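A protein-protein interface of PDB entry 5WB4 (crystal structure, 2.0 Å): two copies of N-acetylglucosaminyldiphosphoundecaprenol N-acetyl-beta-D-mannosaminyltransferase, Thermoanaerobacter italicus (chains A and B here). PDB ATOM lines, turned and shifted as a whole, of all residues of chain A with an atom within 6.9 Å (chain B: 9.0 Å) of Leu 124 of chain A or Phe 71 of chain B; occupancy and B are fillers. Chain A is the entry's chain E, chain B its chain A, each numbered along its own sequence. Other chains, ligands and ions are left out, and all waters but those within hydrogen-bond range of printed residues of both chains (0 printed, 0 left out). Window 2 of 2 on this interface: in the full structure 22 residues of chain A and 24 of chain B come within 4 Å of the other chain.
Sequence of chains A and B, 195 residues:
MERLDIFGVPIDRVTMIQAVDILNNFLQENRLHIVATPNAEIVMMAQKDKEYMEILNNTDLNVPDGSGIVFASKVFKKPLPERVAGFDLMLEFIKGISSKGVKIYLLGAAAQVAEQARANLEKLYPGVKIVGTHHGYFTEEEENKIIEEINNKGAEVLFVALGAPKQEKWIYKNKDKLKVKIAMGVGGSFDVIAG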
ATOM      1  N   PHE A  87       8.458   7.582  24.866  1.00  0.00           N
ATOM      2  CA  PHE A  87       9.822   7.759  24.375  1.00  0.00           C
ATOM      3  C   PHE A  87       9.901   7.500  22.846  1.00  0.00           C
ATOM      4  O   PHE A  87      10.546   8.278  22.124  1.00  0.00           O
ATOM      5  CB  PHE A  87      10.780   6.825  25.125  1.00  0.00           C
ATOM      6  CG  PHE A  87      12.191   6.868  24.598  1.00  0.00           C
ATOM      7  CD1 PHE A  87      13.060   7.900  24.958  1.00  0.00           C
ATOM      8  CD2 PHE A  87      12.649   5.896  23.732  1.00  0.00           C
ATOM      9  CE1 PHE A  87      14.357   7.959  24.432  1.00  0.00           C
ATOM     10  CE2 PHE A  87      13.945   5.955  23.219  1.00  0.00           C
ATOM     11  CZ  PHE A  87      14.787   6.982  23.570  1.00  0.00           C
ATOM     12  N   ASP A  88       9.264   6.401  22.370  1.00  0.00           N
ATOM     13  CA  ASP A  88       9.295   6.032  20.944  1.00  0.00           C
ATOM     14  C   ASP A  88       8.509   7.040  20.127  1.00  0.00           C
ATOM     15  O   ASP A  88       8.920   7.344  19.011  1.00  0.00           O
ATOM     16  CB  ASP A  88       8.736   4.632  20.716  1.00  0.00           C
ATOM     17  CG  ASP A  88       9.485   3.514  21.403  1.00  0.00           C
ATOM     18  OD1 ASP A  88      10.658   3.711  21.759  1.00  0.00           O
ATOM     19  OD2 ASP A  88       8.908   2.439  21.545  1.00  0.00           O
ATOM     20  N   LEU A  91      10.856  10.055  19.566  1.00  0.00           N
ATOM     21  CA  LEU A  91      11.857   9.742  18.540  1.00  0.00           C
ATOM     22  C   LEU A  91      11.273   9.643  17.136  1.00  0.00           C
ATOM     23  O   LEU A  91      11.874  10.169  16.198  1.00  0.00           O
ATOM     24  CB  LEU A  91      12.650   8.470  18.861  1.00  0.00           C
ATOM     25  CG  LEU A  91      13.713   8.538  19.967  1.00  0.00           C
ATOM     26  CD1 LEU A  91      14.564   7.314  19.918  1.00  0.00           C
ATOM     27  CD2 LEU A  91      14.621   9.772  19.830  1.00  0.00           C
ATOM     28  N   LYS A  95      12.214  12.058  14.087  1.00  0.00           N
ATOM     29  CA  LYS A  95      12.661  11.418  12.837  1.00  0.00           C
ATOM     30  C   LYS A  95      11.979  12.060  11.620  1.00  0.00           C
ATOM     31  O   LYS A  95      12.663  12.492  10.697  1.00  0.00           O
ATOM     32  CB  LYS A  95      12.395   9.899  12.884  1.00  0.00           C
ATOM     33  CG  LYS A  95      12.984   9.108  11.706  1.00  0.00           C
ATOM     34  CD  LYS A  95      12.393   7.703  11.658  1.00  0.00           C
ATOM     35  CE  LYS A  95      12.981   6.863  10.550  1.00  0.00           C
ATOM     36  NZ  LYS A  95      14.229   6.179  10.984  1.00  0.00           N
ATOM     37  N   SER A  98      12.877  15.951  11.222  1.00  0.00           N
ATOM     38  CA  SER A  98      14.318  16.226  11.098  1.00  0.00           C
ATOM     39  C   SER A  98      14.766  16.678   9.701  1.00  0.00           C
ATOM     40  O   SER A  98      15.802  17.328   9.582  1.00  0.00           O
ATOM     41  CB  SER A  98      15.149  15.035  11.565  1.00  0.00           C
ATOM     42  OG  SER A  98      14.991  13.915  10.716  1.00  0.00           O
ATOM     43  N   ALA A 117      22.109  15.216  24.692  1.00  0.00           N
ATOM     44  CA  ALA A 117      20.943  14.676  23.968  1.00  0.00           C
ATOM     45  C   ALA A 117      20.872  15.317  22.575  1.00  0.00           C
ATOM     46  O   ALA A 117      20.674  14.609  21.590  1.00  0.00           O
ATOM     47  CB  ALA A 117      19.652  14.958  24.739  1.00  0.00           C
ATOM     48  N   ALA A 119      23.432  16.742  20.813  1.00  0.00           N
ATOM     49  CA  ALA A 119      24.566  16.212  20.052  1.00  0.00           C
ATOM     50  C   ALA A 119      24.245  14.829  19.476  1.00  0.00           C
ATOM     51  O   ALA A 119      24.475  14.598  18.284  1.00  0.00           O
ATOM     52  CB  ALA A 119      25.806  16.151  20.933  1.00  0.00           C
ATOM     53  N   ASN A 120      23.640  13.939  20.302  1.00  0.00           N
ATOM     54  CA  ASN A 120      23.290  12.579  19.890  1.00  0.00           C
ATOM     55  C   ASN A 120      22.134  12.534  18.879  1.00  0.00           C
ATOM     56  O   ASN A 120      22.195  11.742  17.933  1.00  0.00           O
ATOM     57  CB  ASN A 120      23.047  11.688  21.109  1.00  0.00           C
ATOM     58  CG  ASN A 120      24.327  11.453  21.903  1.00  0.00           C
ATOM     59  OD1 ASN A 120      25.421  11.870  21.501  1.00  0.00           O
ATOM     60  ND2 ASN A 120      24.236  10.818  23.068  1.00  0.00           N
ATOM     61  N   LEU A 121      21.130  13.419  19.026  1.00  0.00           N
ATOM     62  CA  LEU A 121      20.012  13.499  18.079  1.00  0.00           C
ATOM     63  C   LEU A 121      20.465  14.030  16.724  1.00  0.00           C
ATOM     64  O   LEU A 121      19.939  13.604  15.691  1.00  0.00           O
ATOM     65  CB  LEU A 121      18.875  14.376  18.635  1.00  0.00           C
ATOM     66  CG  LEU A 121      18.031  13.769  19.760  1.00  0.00           C
ATOM     67  CD1 LEU A 121      17.282  14.859  20.499  1.00  0.00           C
ATOM     68  CD2 LEU A 121      17.070  12.709  19.232  1.00  0.00           C
ATOM     69  N   GLU A 122      21.484  14.915  16.720  1.00  0.00           N
ATOM     70  CA  GLU A 122      22.050  15.460  15.480  1.00  0.00           C
ATOM     71  C   GLU A 122      22.783  14.371  14.686  1.00  0.00           C
ATOM     72  O   GLU A 122      22.779  14.422  13.452  1.00  0.00           O
ATOM     73  CB  GLU A 122      22.963  16.664  15.760  1.00  0.00           C
ATOM     74  CG  GLU A 122      22.187  17.922  16.125  1.00  0.00           C
ATOM     75  CD  GLU A 122      23.014  19.033  16.740  1.00  0.00           C
ATOM     76  OE1 GLU A 122      24.203  18.803  17.068  1.00  0.00           O
ATOM     77  OE2 GLU A 122      22.462  20.144  16.899  1.00  0.00           O
ATOM     78  N   LYS A 123      23.395  13.386  15.396  1.00  0.00           N
ATOM     79  CA  LYS A 123      24.068  12.231  14.792  1.00  0.00           C
ATOM     80  C   LYS A 123      23.024  11.233  14.280  1.00  0.00           C
ATOM     81  O   LYS A 123      23.172  10.719  13.174  1.00  0.00           O
ATOM     82  CB  LYS A 123      25.004  11.533  15.802  1.00  0.00           C
ATOM     83  CG  LYS A 123      26.307  12.289  16.058  1.00  0.00           C
ATOM     84  CD  LYS A 123      27.185  11.598  17.095  1.00  0.00           C
ATOM     85  CE  LYS A 123      28.404  12.416  17.471  1.00  0.00           C
ATOM     86  NZ  LYS A 123      29.412  12.468  16.376  1.00  0.00           N
ATOM     87  N   LEU A 124      21.983  10.949  15.094  1.00  0.00           N
ATOM     88  CA  LEU A 124      20.915   9.996  14.778  1.00  0.00           C
ATOM     89  C   LEU A 124      20.018  10.459  13.638  1.00  0.00           C
ATOM     90  O   LEU A 124      19.605   9.638  12.822  1.00  0.00           O
ATOM     91  CB  LEU A 124      20.041   9.719  16.017  1.00  0.00           C
ATOM     92  CG  LEU A 124      20.624   8.797  17.088  1.00  0.00           C
ATOM     93  CD1 LEU A 124      19.889   8.970  18.400  1.00  0.00           C
ATOM     94  CD2 LEU A 124      20.597   7.325  16.636  1.00  0.00           C
ATOM     95  N   TYR A 125      19.670  11.752  13.621  1.00  0.00           N
ATOM     96  CA  TYR A 125      18.784  12.318  12.613  1.00  0.00           C
ATOM     97  C   TYR A 125      19.474  13.500  11.924  1.00  0.00           C
ATOM     98  O   TYR A 125      19.226  14.651  12.294  1.00  0.00           O
ATOM     99  CB  TYR A 125      17.423  12.697  13.235  1.00  0.00           C
ATOM    100  CG  TYR A 125      16.792  11.576  14.038  1.00  0.00           C
ATOM    101  CD1 TYR A 125      16.309  10.427  13.411  1.00  0.00           C
ATOM    102  CD2 TYR A 125      16.740  11.631  15.428  1.00  0.00           C
ATOM    103  CE1 TYR A 125      15.769   9.373  14.146  1.00  0.00           C
ATOM    104  CE2 TYR A 125      16.191  10.588  16.174  1.00  0.00           C
ATOM    105  CZ  TYR A 125      15.693   9.469  15.528  1.00  0.00           C
ATOM    106  OH  TYR A 125      15.154   8.447  16.263  1.00  0.00           O
ATOM    107  N   PRO A 126      20.366  13.230  10.930  1.00  0.00           N
ATOM    108  CA  PRO A 126      21.062  14.338  10.248  1.00  0.00           C
ATOM    109  C   PRO A 126      20.095  15.353   9.644  1.00  0.00           C
ATOM    110  O   PRO A 126      19.105  14.975   9.009  1.00  0.00           O
ATOM    111  CB  PRO A 126      21.915  13.629   9.186  1.00  0.00           C
ATOM    112  CG  PRO A 126      22.082  12.242   9.693  1.00  0.00           C
ATOM    113  CD  PRO A 126      20.785  11.923  10.381  1.00  0.00           C
ATOM    114  N   VAL A 128      18.427  17.545  11.662  1.00  0.00           N
ATOM    115  CA  VAL A 128      17.558  17.961  12.772  1.00  0.00           C
ATOM    116  C   VAL A 128      17.951  19.367  13.255  1.00  0.00           C
ATOM    117  O   VAL A 128      19.142  19.683  13.379  1.00  0.00           O
ATOM    118  CB  VAL A 128      17.435  16.922  13.922  1.00  0.00           C
ATOM    119  CG1 VAL A 128      18.696  16.854  14.793  1.00  0.00           C
ATOM    120  CG2 VAL A 128      16.190  17.177  14.777  1.00  0.00           C
ATOM    121  N   SER A 189      13.566  10.980  29.157  1.00  0.00           N
ATOM    122  CA  SER A 189      13.942  10.768  27.749  1.00  0.00           C
ATOM    123  C   SER A 189      15.279  11.397  27.328  1.00  0.00           C
ATOM    124  O   SER A 189      15.942  10.818  26.478  1.00  0.00           O
ATOM    125  CB  SER A 189      12.831  11.211  26.798  1.00  0.00           C
ATOM    126  OG  SER A 189      11.670  10.396  26.920  1.00  0.00           O
ATOM    127  N   VAL A 192      18.459   9.105  28.719  1.00  0.00           N
ATOM    128  CA  VAL A 192      18.660   7.864  27.966  1.00  0.00           C
ATOM    129  C   VAL A 192      19.146   8.103  26.514  1.00  0.00           C
ATOM    130  O   VAL A 192      19.631   7.170  25.894  1.00  0.00           O
ATOM    131  CB  VAL A 192      17.420   6.940  28.033  1.00  0.00           C
ATOM    132  CG1 VAL A 192      17.242   6.367  29.433  1.00  0.00           C
ATOM    133  CG2 VAL A 192      16.155   7.646  27.552  1.00  0.00           C
ATOM    134  N   ILE A 193      18.986   9.323  25.964  1.00  0.00           N
ATOM    135  CA  ILE A 193      19.487   9.682  24.629  1.00  0.00           C
ATOM    136  C   ILE A 193      20.923  10.221  24.798  1.00  0.00           C
ATOM    137  O   ILE A 193      21.726  10.148  23.869  1.00  0.00           O
ATOM    138  CB  ILE A 193      18.579  10.691  23.875  1.00  0.00           C
ATOM    139  CG1 ILE A 193      17.189  10.117  23.572  1.00  0.00           C
ATOM    140  CG2 ILE A 193      19.238  11.251  22.589  1.00  0.00           C
ATOM    141  CD1 ILE A 193      16.213  11.207  23.139  1.00  0.00           C
ATOM    142  N   ALA A 194      21.211  10.771  25.986  1.00  0.00           N
ATOM    143  CA  ALA A 194      22.525  11.279  26.382  1.00  0.00           C
ATOM    144  C   ALA A 194      23.370  10.113  26.880  1.00  0.00           C
ATOM    145  O   ALA A 194      24.521   9.968  26.478  1.00  0.00           O
ATOM    146  CB  ALA A 194      22.374  12.315  27.489  1.00  0.00           C
ATOM    147  N   ILE B   6      23.654   2.182  33.897  1.00  0.00           N
ATOM    148  CA  ILE B   6      22.989   3.292  33.210  1.00  0.00           C
ATOM    149  C   ILE B   6      23.066   4.484  34.169  1.00  0.00           C
ATOM    150  O   ILE B   6      22.263   4.590  35.099  1.00  0.00           O
ATOM    151  CB  ILE B   6      21.520   2.937  32.776  1.00  0.00           C
ATOM    152  CG1 ILE B   6      21.442   1.634  31.897  1.00  0.00           C
ATOM    153  CG2 ILE B   6      20.803   4.136  32.084  1.00  0.00           C
ATOM    154  CD1 ILE B   6      22.079   1.683  30.462  1.00  0.00           C
ATOM    155  N   PHE B   7      24.091   5.345  33.978  1.00  0.00           N
ATOM    156  CA  PHE B   7      24.360   6.545  34.773  1.00  0.00           C
ATOM    157  C   PHE B   7      24.365   6.270  36.282  1.00  0.00           C
ATOM    158  O   PHE B   7      23.711   6.981  37.048  1.00  0.00           O
ATOM    159  CB  PHE B   7      23.399   7.688  34.384  1.00  0.00           C
ATOM    160  CG  PHE B   7      23.460   8.028  32.911  1.00  0.00           C
ATOM    161  CD1 PHE B   7      24.501   8.801  32.398  1.00  0.00           C
ATOM    162  CD2 PHE B   7      22.501   7.542  32.029  1.00  0.00           C
ATOM    163  CE1 PHE B   7      24.584   9.067  31.029  1.00  0.00           C
ATOM    164  CE2 PHE B   7      22.576   7.830  30.664  1.00  0.00           C
ATOM    165  CZ  PHE B   7      23.614   8.592  30.177  1.00  0.00           C
ATOM    166  N   ALA B  40      13.721   5.148  32.389  1.00  0.00           N
ATOM    167  CA  ALA B  40      14.412   6.415  32.106  1.00  0.00           C
ATOM    168  C   ALA B  40      14.160   7.474  33.208  1.00  0.00           C
ATOM    169  O   ALA B  40      15.111   8.110  33.675  1.00  0.00           O
ATOM    170  CB  ALA B  40      13.968   6.946  30.748  1.00  0.00           C
ATOM    171  N   PRO B  64      14.813  -3.959  33.663  1.00  0.00           N
ATOM    172  CA  PRO B  64      14.563  -2.725  32.905  1.00  0.00           C
ATOM    173  C   PRO B  64      13.072  -2.520  32.654  1.00  0.00           C
ATOM    174  O   PRO B  64      12.338  -3.483  32.407  1.00  0.00           O
ATOM    175  CB  PRO B  64      15.327  -2.951  31.593  1.00  0.00           C
ATOM    176  CG  PRO B  64      15.405  -4.435  31.445  1.00  0.00           C
ATOM    177  CD  PRO B  64      15.571  -4.936  32.854  1.00  0.00           C
ATOM    178  N   ASP B  65      12.618  -1.266  32.750  1.00  0.00           N
ATOM    179  CA  ASP B  65      11.228  -0.928  32.472  1.00  0.00           C
ATOM    180  C   ASP B  65      11.169   0.132  31.368  1.00  0.00           C
ATOM    181  O   ASP B  65      11.897   1.097  31.427  1.00  0.00           O
ATOM    182  CB  ASP B  65      10.484  -0.464  33.759  1.00  0.00           C
ATOM    183  CG  ASP B  65       9.105   0.082  33.471  1.00  0.00           C
ATOM    184  OD1 ASP B  65       8.254  -0.691  32.970  1.00  0.00           O
ATOM    185  OD2 ASP B  65       8.909   1.309  33.626  1.00  0.00           O
ATOM    186  N   GLY B  66      10.311  -0.070  30.375  1.00  0.00           N
ATOM    187  CA  GLY B  66      10.111   0.873  29.287  1.00  0.00           C
ATOM    188  C   GLY B  66      11.123   0.794  28.159  1.00  0.00           C
ATOM    189  O   GLY B  66      12.033  -0.037  28.160  1.00  0.00           O
ATOM    190  N   SER B  67      10.974   1.699  27.194  1.00  0.00           N
ATOM    191  CA  SER B  67      11.791   1.747  25.991  1.00  0.00           C
ATOM    192  C   SER B  67      13.080   2.569  26.129  1.00  0.00           C
ATOM    193  O   SER B  67      14.112   2.166  25.580  1.00  0.00           O
ATOM    194  CB  SER B  67      10.962   2.301  24.833  1.00  0.00           C
ATOM    195  OG  SER B  67      11.700   2.139  23.640  1.00  0.00           O
ATOM    196  N   GLY B  68      12.981   3.721  26.806  1.00  0.00           N
ATOM    197  CA  GLY B  68      14.078   4.654  27.018  1.00  0.00           C
ATOM    198  C   GLY B  68      15.334   3.994  27.550  1.00  0.00           C
ATOM    199  O   GLY B  68      16.409   4.183  26.975  1.00  0.00           O
ATOM    200  N   ILE B  69      15.198   3.173  28.624  1.00  0.00           N
ATOM    201  CA  ILE B  69      16.343   2.511  29.257  1.00  0.00           C
ATOM    202  C   ILE B  69      17.012   1.511  28.291  1.00  0.00           C
ATOM    203  O   ILE B  69      18.240   1.389  28.299  1.00  0.00           O
ATOM    204  CB  ILE B  69      15.994   1.920  30.650  1.00  0.00           C
ATOM    205  CG1 ILE B  69      17.272   1.752  31.518  1.00  0.00           C
ATOM    206  CG2 ILE B  69      15.145   0.637  30.579  1.00  0.00           C
ATOM    207  CD1 ILE B  69      17.050   1.970  32.981  1.00  0.00           C
ATOM    208  N   VAL B  70      16.224   0.840  27.449  1.00  0.00           N
ATOM    209  CA  VAL B  70      16.746  -0.101  26.443  1.00  0.00           C
ATOM    210  C   VAL B  70      17.547   0.698  25.388  1.00  0.00           C
ATOM    211  O   VAL B  70      18.660   0.314  25.036  1.00  0.00           O
ATOM    212  CB  VAL B  70      15.602  -0.955  25.834  1.00  0.00           C
ATOM    213  CG1 VAL B  70      16.115  -1.807  24.663  1.00  0.00           C
ATOM    214  CG2 VAL B  70      14.980  -1.845  26.916  1.00  0.00           C
ATOM    215  N   PHE B  71      16.993   1.836  24.925  1.00  0.00           N
ATOM    216  CA  PHE B  71      17.687   2.698  23.965  1.00  0.00           C
ATOM    217  C   PHE B  71      19.061   3.155  24.533  1.00  0.00           C
ATOM    218  O   PHE B  71      20.050   3.094  23.808  1.00  0.00           O
ATOM    219  CB  PHE B  71      16.810   3.913  23.596  1.00  0.00           C
ATOM    220  CG  PHE B  71      17.382   4.780  22.498  1.00  0.00           C
ATOM    221  CD1 PHE B  71      17.109   4.511  21.162  1.00  0.00           C
ATOM    222  CD2 PHE B  71      18.199   5.870  22.799  1.00  0.00           C
ATOM    223  CE1 PHE B  71      17.661   5.302  20.140  1.00  0.00           C
ATOM    224  CE2 PHE B  71      18.720   6.681  21.781  1.00  0.00           C
ATOM    225  CZ  PHE B  71      18.452   6.388  20.458  1.00  0.00           C
ATOM    226  N   ALA B  72      19.112   3.576  25.828  1.00  0.00           N
ATOM    227  CA  ALA B  72      20.355   3.980  26.493  1.00  0.00           C
ATOM    228  C   ALA B  72      21.414   2.852  26.469  1.00  0.00           C
ATOM    229  O   ALA B  72      22.594   3.139  26.314  1.00  0.00           O
ATOM    230  CB  ALA B  72      20.080   4.380  27.940  1.00  0.00           C
ATOM    231  N   SER B  73      20.978   1.574  26.594  1.00  0.00           N
ATOM    232  CA  SER B  73      21.857   0.420  26.613  1.00  0.00           C
ATOM    233  C   SER B  73      22.493   0.094  25.259  1.00  0.00           C
ATOM    234  O   SER B  73      23.438  -0.695  25.239  1.00  0.00           O
ATOM    235  CB  SER B  73      21.133  -0.803  27.176  1.00  0.00           C
ATOM    236  OG  SER B  73      20.338  -1.460  26.198  1.00  0.00           O
ATOM    237  N   LYS B  74      21.987   0.686  24.144  1.00  0.00           N
ATOM    238  CA  LYS B  74      22.519   0.437  22.790  1.00  0.00           C
ATOM    239  C   LYS B  74      24.001   0.836  22.631  1.00  0.00           C
ATOM    240  O   LYS B  74      24.661   0.336  21.714  1.00  0.00           O
ATOM    241  CB  LYS B  74      21.671   1.134  21.712  1.00  0.00           C
ATOM    242  CG  LYS B  74      20.218   0.643  21.606  1.00  0.00           C
ATOM    243  CD  LYS B  74      19.420   1.507  20.647  1.00  0.00           C
ATOM    244  CE  LYS B  74      19.081   0.773  19.379  1.00  0.00           C
ATOM    245  NZ  LYS B  74      18.373   1.656  18.417  1.00  0.00           N
ATOM    246  N   VAL B  75      24.521   1.701  23.529  1.00  0.00           N
ATOM    247  CA  VAL B  75      25.929   2.144  23.532  1.00  0.00           C
ATOM    248  C   VAL B  75      26.892   0.982  23.912  1.00  0.00           C
ATOM    249  O   VAL B  75      28.098   1.077  23.658  1.00  0.00           O
ATOM    250  CB  VAL B  75      26.167   3.398  24.426  1.00  0.00           C
ATOM    251  CG1 VAL B  75      25.371   4.606  23.934  1.00  0.00           C
ATOM    252  CG2 VAL B  75      25.881   3.117  25.904  1.00  0.00           C
ATOM    253  N   PHE B  76      26.349  -0.084  24.547  1.00  0.00           N
ATOM    254  CA  PHE B  76      27.123  -1.237  25.001  1.00  0.00           C
ATOM    255  C   PHE B  76      27.241  -2.315  23.943  1.00  0.00           C
ATOM    256  O   PHE B  76      26.315  -2.487  23.168  1.00  0.00           O
ATOM    257  CB  PHE B  76      26.496  -1.831  26.262  1.00  0.00           C
ATOM    258  CG  PHE B  76      26.512  -0.903  27.451  1.00  0.00           C
ATOM    259  CD1 PHE B  76      27.627  -0.817  28.268  1.00  0.00           C
ATOM    260  CD2 PHE B  76      25.391  -0.160  27.785  1.00  0.00           C
ATOM    261  CE1 PHE B  76      27.625   0.003  29.392  1.00  0.00           C
ATOM    262  CE2 PHE B  76      25.403   0.692  28.889  1.00  0.00           C
ATOM    263  CZ  PHE B  76      26.517   0.759  29.691  1.00  0.00           C
ATOM    264  N   PRO B  79      23.815  -4.922  24.714  1.00  0.00           N
ATOM    265  CA  PRO B  79      22.721  -4.089  25.238  1.00  0.00           C
ATOM    266  C   PRO B  79      21.707  -4.911  26.041  1.00  0.00           C
ATOM    267  O   PRO B  79      21.837  -6.144  26.134  1.00  0.00           O
ATOM    268  CB  PRO B  79      22.091  -3.474  23.962  1.00  0.00           C
ATOM    269  CG  PRO B  79      23.038  -3.830  22.811  1.00  0.00           C
ATOM    270  CD  PRO B  79      23.690  -5.110  23.253  1.00  0.00           C
ATOM    271  N   LEU B  80      20.684  -4.226  26.612  1.00  0.00           N
ATOM    272  CA  LEU B  80      19.592  -4.910  27.317  1.00  0.00           C
ATOM    273  C   LEU B  80      18.834  -5.748  26.234  1.00  0.00           C
ATOM    274  O   LEU B  80      18.651  -5.244  25.119  1.00  0.00           O
ATOM    275  CB  LEU B  80      18.677  -3.901  28.042  1.00  0.00           C
ATOM    276  CG  LEU B  80      19.331  -3.166  29.247  1.00  0.00           C
ATOM    277  CD1 LEU B  80      18.472  -2.015  29.746  1.00  0.00           C
ATOM    278  CD2 LEU B  80      19.702  -4.124  30.383  1.00  0.00           C
ATOM    279  N   GLU B  82      15.716  -6.970  25.797  1.00  0.00           N
ATOM    280  CA  GLU B  82      14.364  -6.627  25.373  1.00  0.00           C
ATOM    281  C   GLU B  82      13.643  -5.585  26.218  1.00  0.00           C
ATOM    282  O   GLU B  82      13.970  -5.377  27.396  1.00  0.00           O
ATOM    283  CB  GLU B  82      13.477  -7.865  25.230  1.00  0.00           C
ATOM    284  CG  GLU B  82      13.144  -8.589  26.502  1.00  0.00           C
ATOM    285  CD  GLU B  82      12.339  -9.860  26.305  1.00  0.00           C
ATOM    286  OE1 GLU B  82      12.653 -10.646  25.381  1.00  0.00           O
ATOM    287  OE2 GLU B  82      11.432 -10.102  27.129  1.00  0.00           O
ATOM    288  N   ARG B  83      12.623  -4.962  25.602  1.00  0.00           N
ATOM    289  CA  ARG B  83      11.755  -3.997  26.265  1.00  0.00           C
ATOM    290  C   ARG B  83      10.794  -4.772  27.137  1.00  0.00           C
ATOM    291  O   ARG B  83      10.111  -5.680  26.670  1.00  0.00           O
ATOM    292  CB  ARG B  83      11.011  -3.118  25.239  1.00  0.00           C
ATOM    293  CG  ARG B  83      11.959  -2.064  24.638  1.00  0.00           C
ATOM    294  CD  ARG B  83      11.478  -1.400  23.353  1.00  0.00           C
ATOM    295  NE  ARG B  83      12.475  -0.463  22.836  1.00  0.00           N
ATOM    296  CZ  ARG B  83      13.541  -0.804  22.108  1.00  0.00           C
ATOM    297  NH1 ARG B  83      13.742  -2.071  21.762  1.00  0.00           N
ATOM    298  NH2 ARG B  83      14.408   0.124  21.716  1.00  0.00           N
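Of the 20 printed residues of chain B, 7 touch a printed residue of chain A.
Along chain B the printed residues that touch a printed residue of chain A span positions 7 to 72.
Of the 19 printed residues of chain A, 6 touch a printed residue of chain B.
Printed residues of chain A that touch a printed residue of chain B: Phe 87, Asp 88, Leu 91, Leu 124, Val 192 and Ala 194.
Hydrophobic or aromatic side chains of chain A that line the printed part of chain B: Phe 87, Leu 91, Leu 124 and Val 192.
Among the printed residues, no Asp or Glu carboxylate lies within 4 Å of a Lys or Arg side-chain nitrogen of the other chain.
The guanidinium group of Arg 83 of chain B sits at hydrogen-bond distance from the side-chain hydroxyl of Ser 67 of chain B.
Among the printed residues, pairs that only touch across the chains: Phe 87 of chain A with Ser 67 of chain B (3.9 Å), Phe 87 of chain A with Gly 68 of chain B (3.8 Å), Phe 87 of chain A with Phe 71 of chain B (3.5 Å), Leu 91 of chain A with Phe 71 of chain B (3.7 Å), Leu 124 of chain A with Phe 71 of chain B (3.6 Å), Val 192 of chain A with Ala 40 of chain B (3.6 Å), Val 192 of chain A with Gly 68 of chain B (3.1 Å), Val 192 of chain A with Ile 69 of chain B (3.9 Å), Val 192 of chain A with Phe 71 of chain B (3.6 Å), Val 192 of chain A with Ala 72 of chain B (3.3 Å) and Ala 194 of chain A with Phe 7 of chain B (3.6 Å).
Of the printed residues of chain B, Asp 88 of chain A touches Ser 67 (2.7 Å).
Leu 124 of chain A touches one residue of chain B.
Printed residues of chain A within 4 Å of Ala 40 of chain B: Val 192.
Gly 66 of chain B touches none of the printed residues of chain A.
Printed residues of chain A within 4 Å of Gly 68 of chain B: Phe 87 (3.8 Å) and Val 192 (3.1 Å).
Of chain A, only Phe 87, Leu 91, Leu 124 and Val 192 come within 4 Å of Phe 71 of chain B.
Ser 73 of chain B touches none of the printed residues of chain A.
The nearest residue of chain B that does not touch Leu 124 of chain A is Lys 74 of chain B (6.3 Å).
No position is printed for both chains.
Of the 12 pairs that touch across the chains among the printed residues, none has its exchanged pair printed and touching as well.
The side-chain carboxylate (OD1) of Asp 88 of chain A lies within hydrogen-bond range of the side-chain hydroxyl (OG) of Ser 67 of chain B (2.7 Å).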
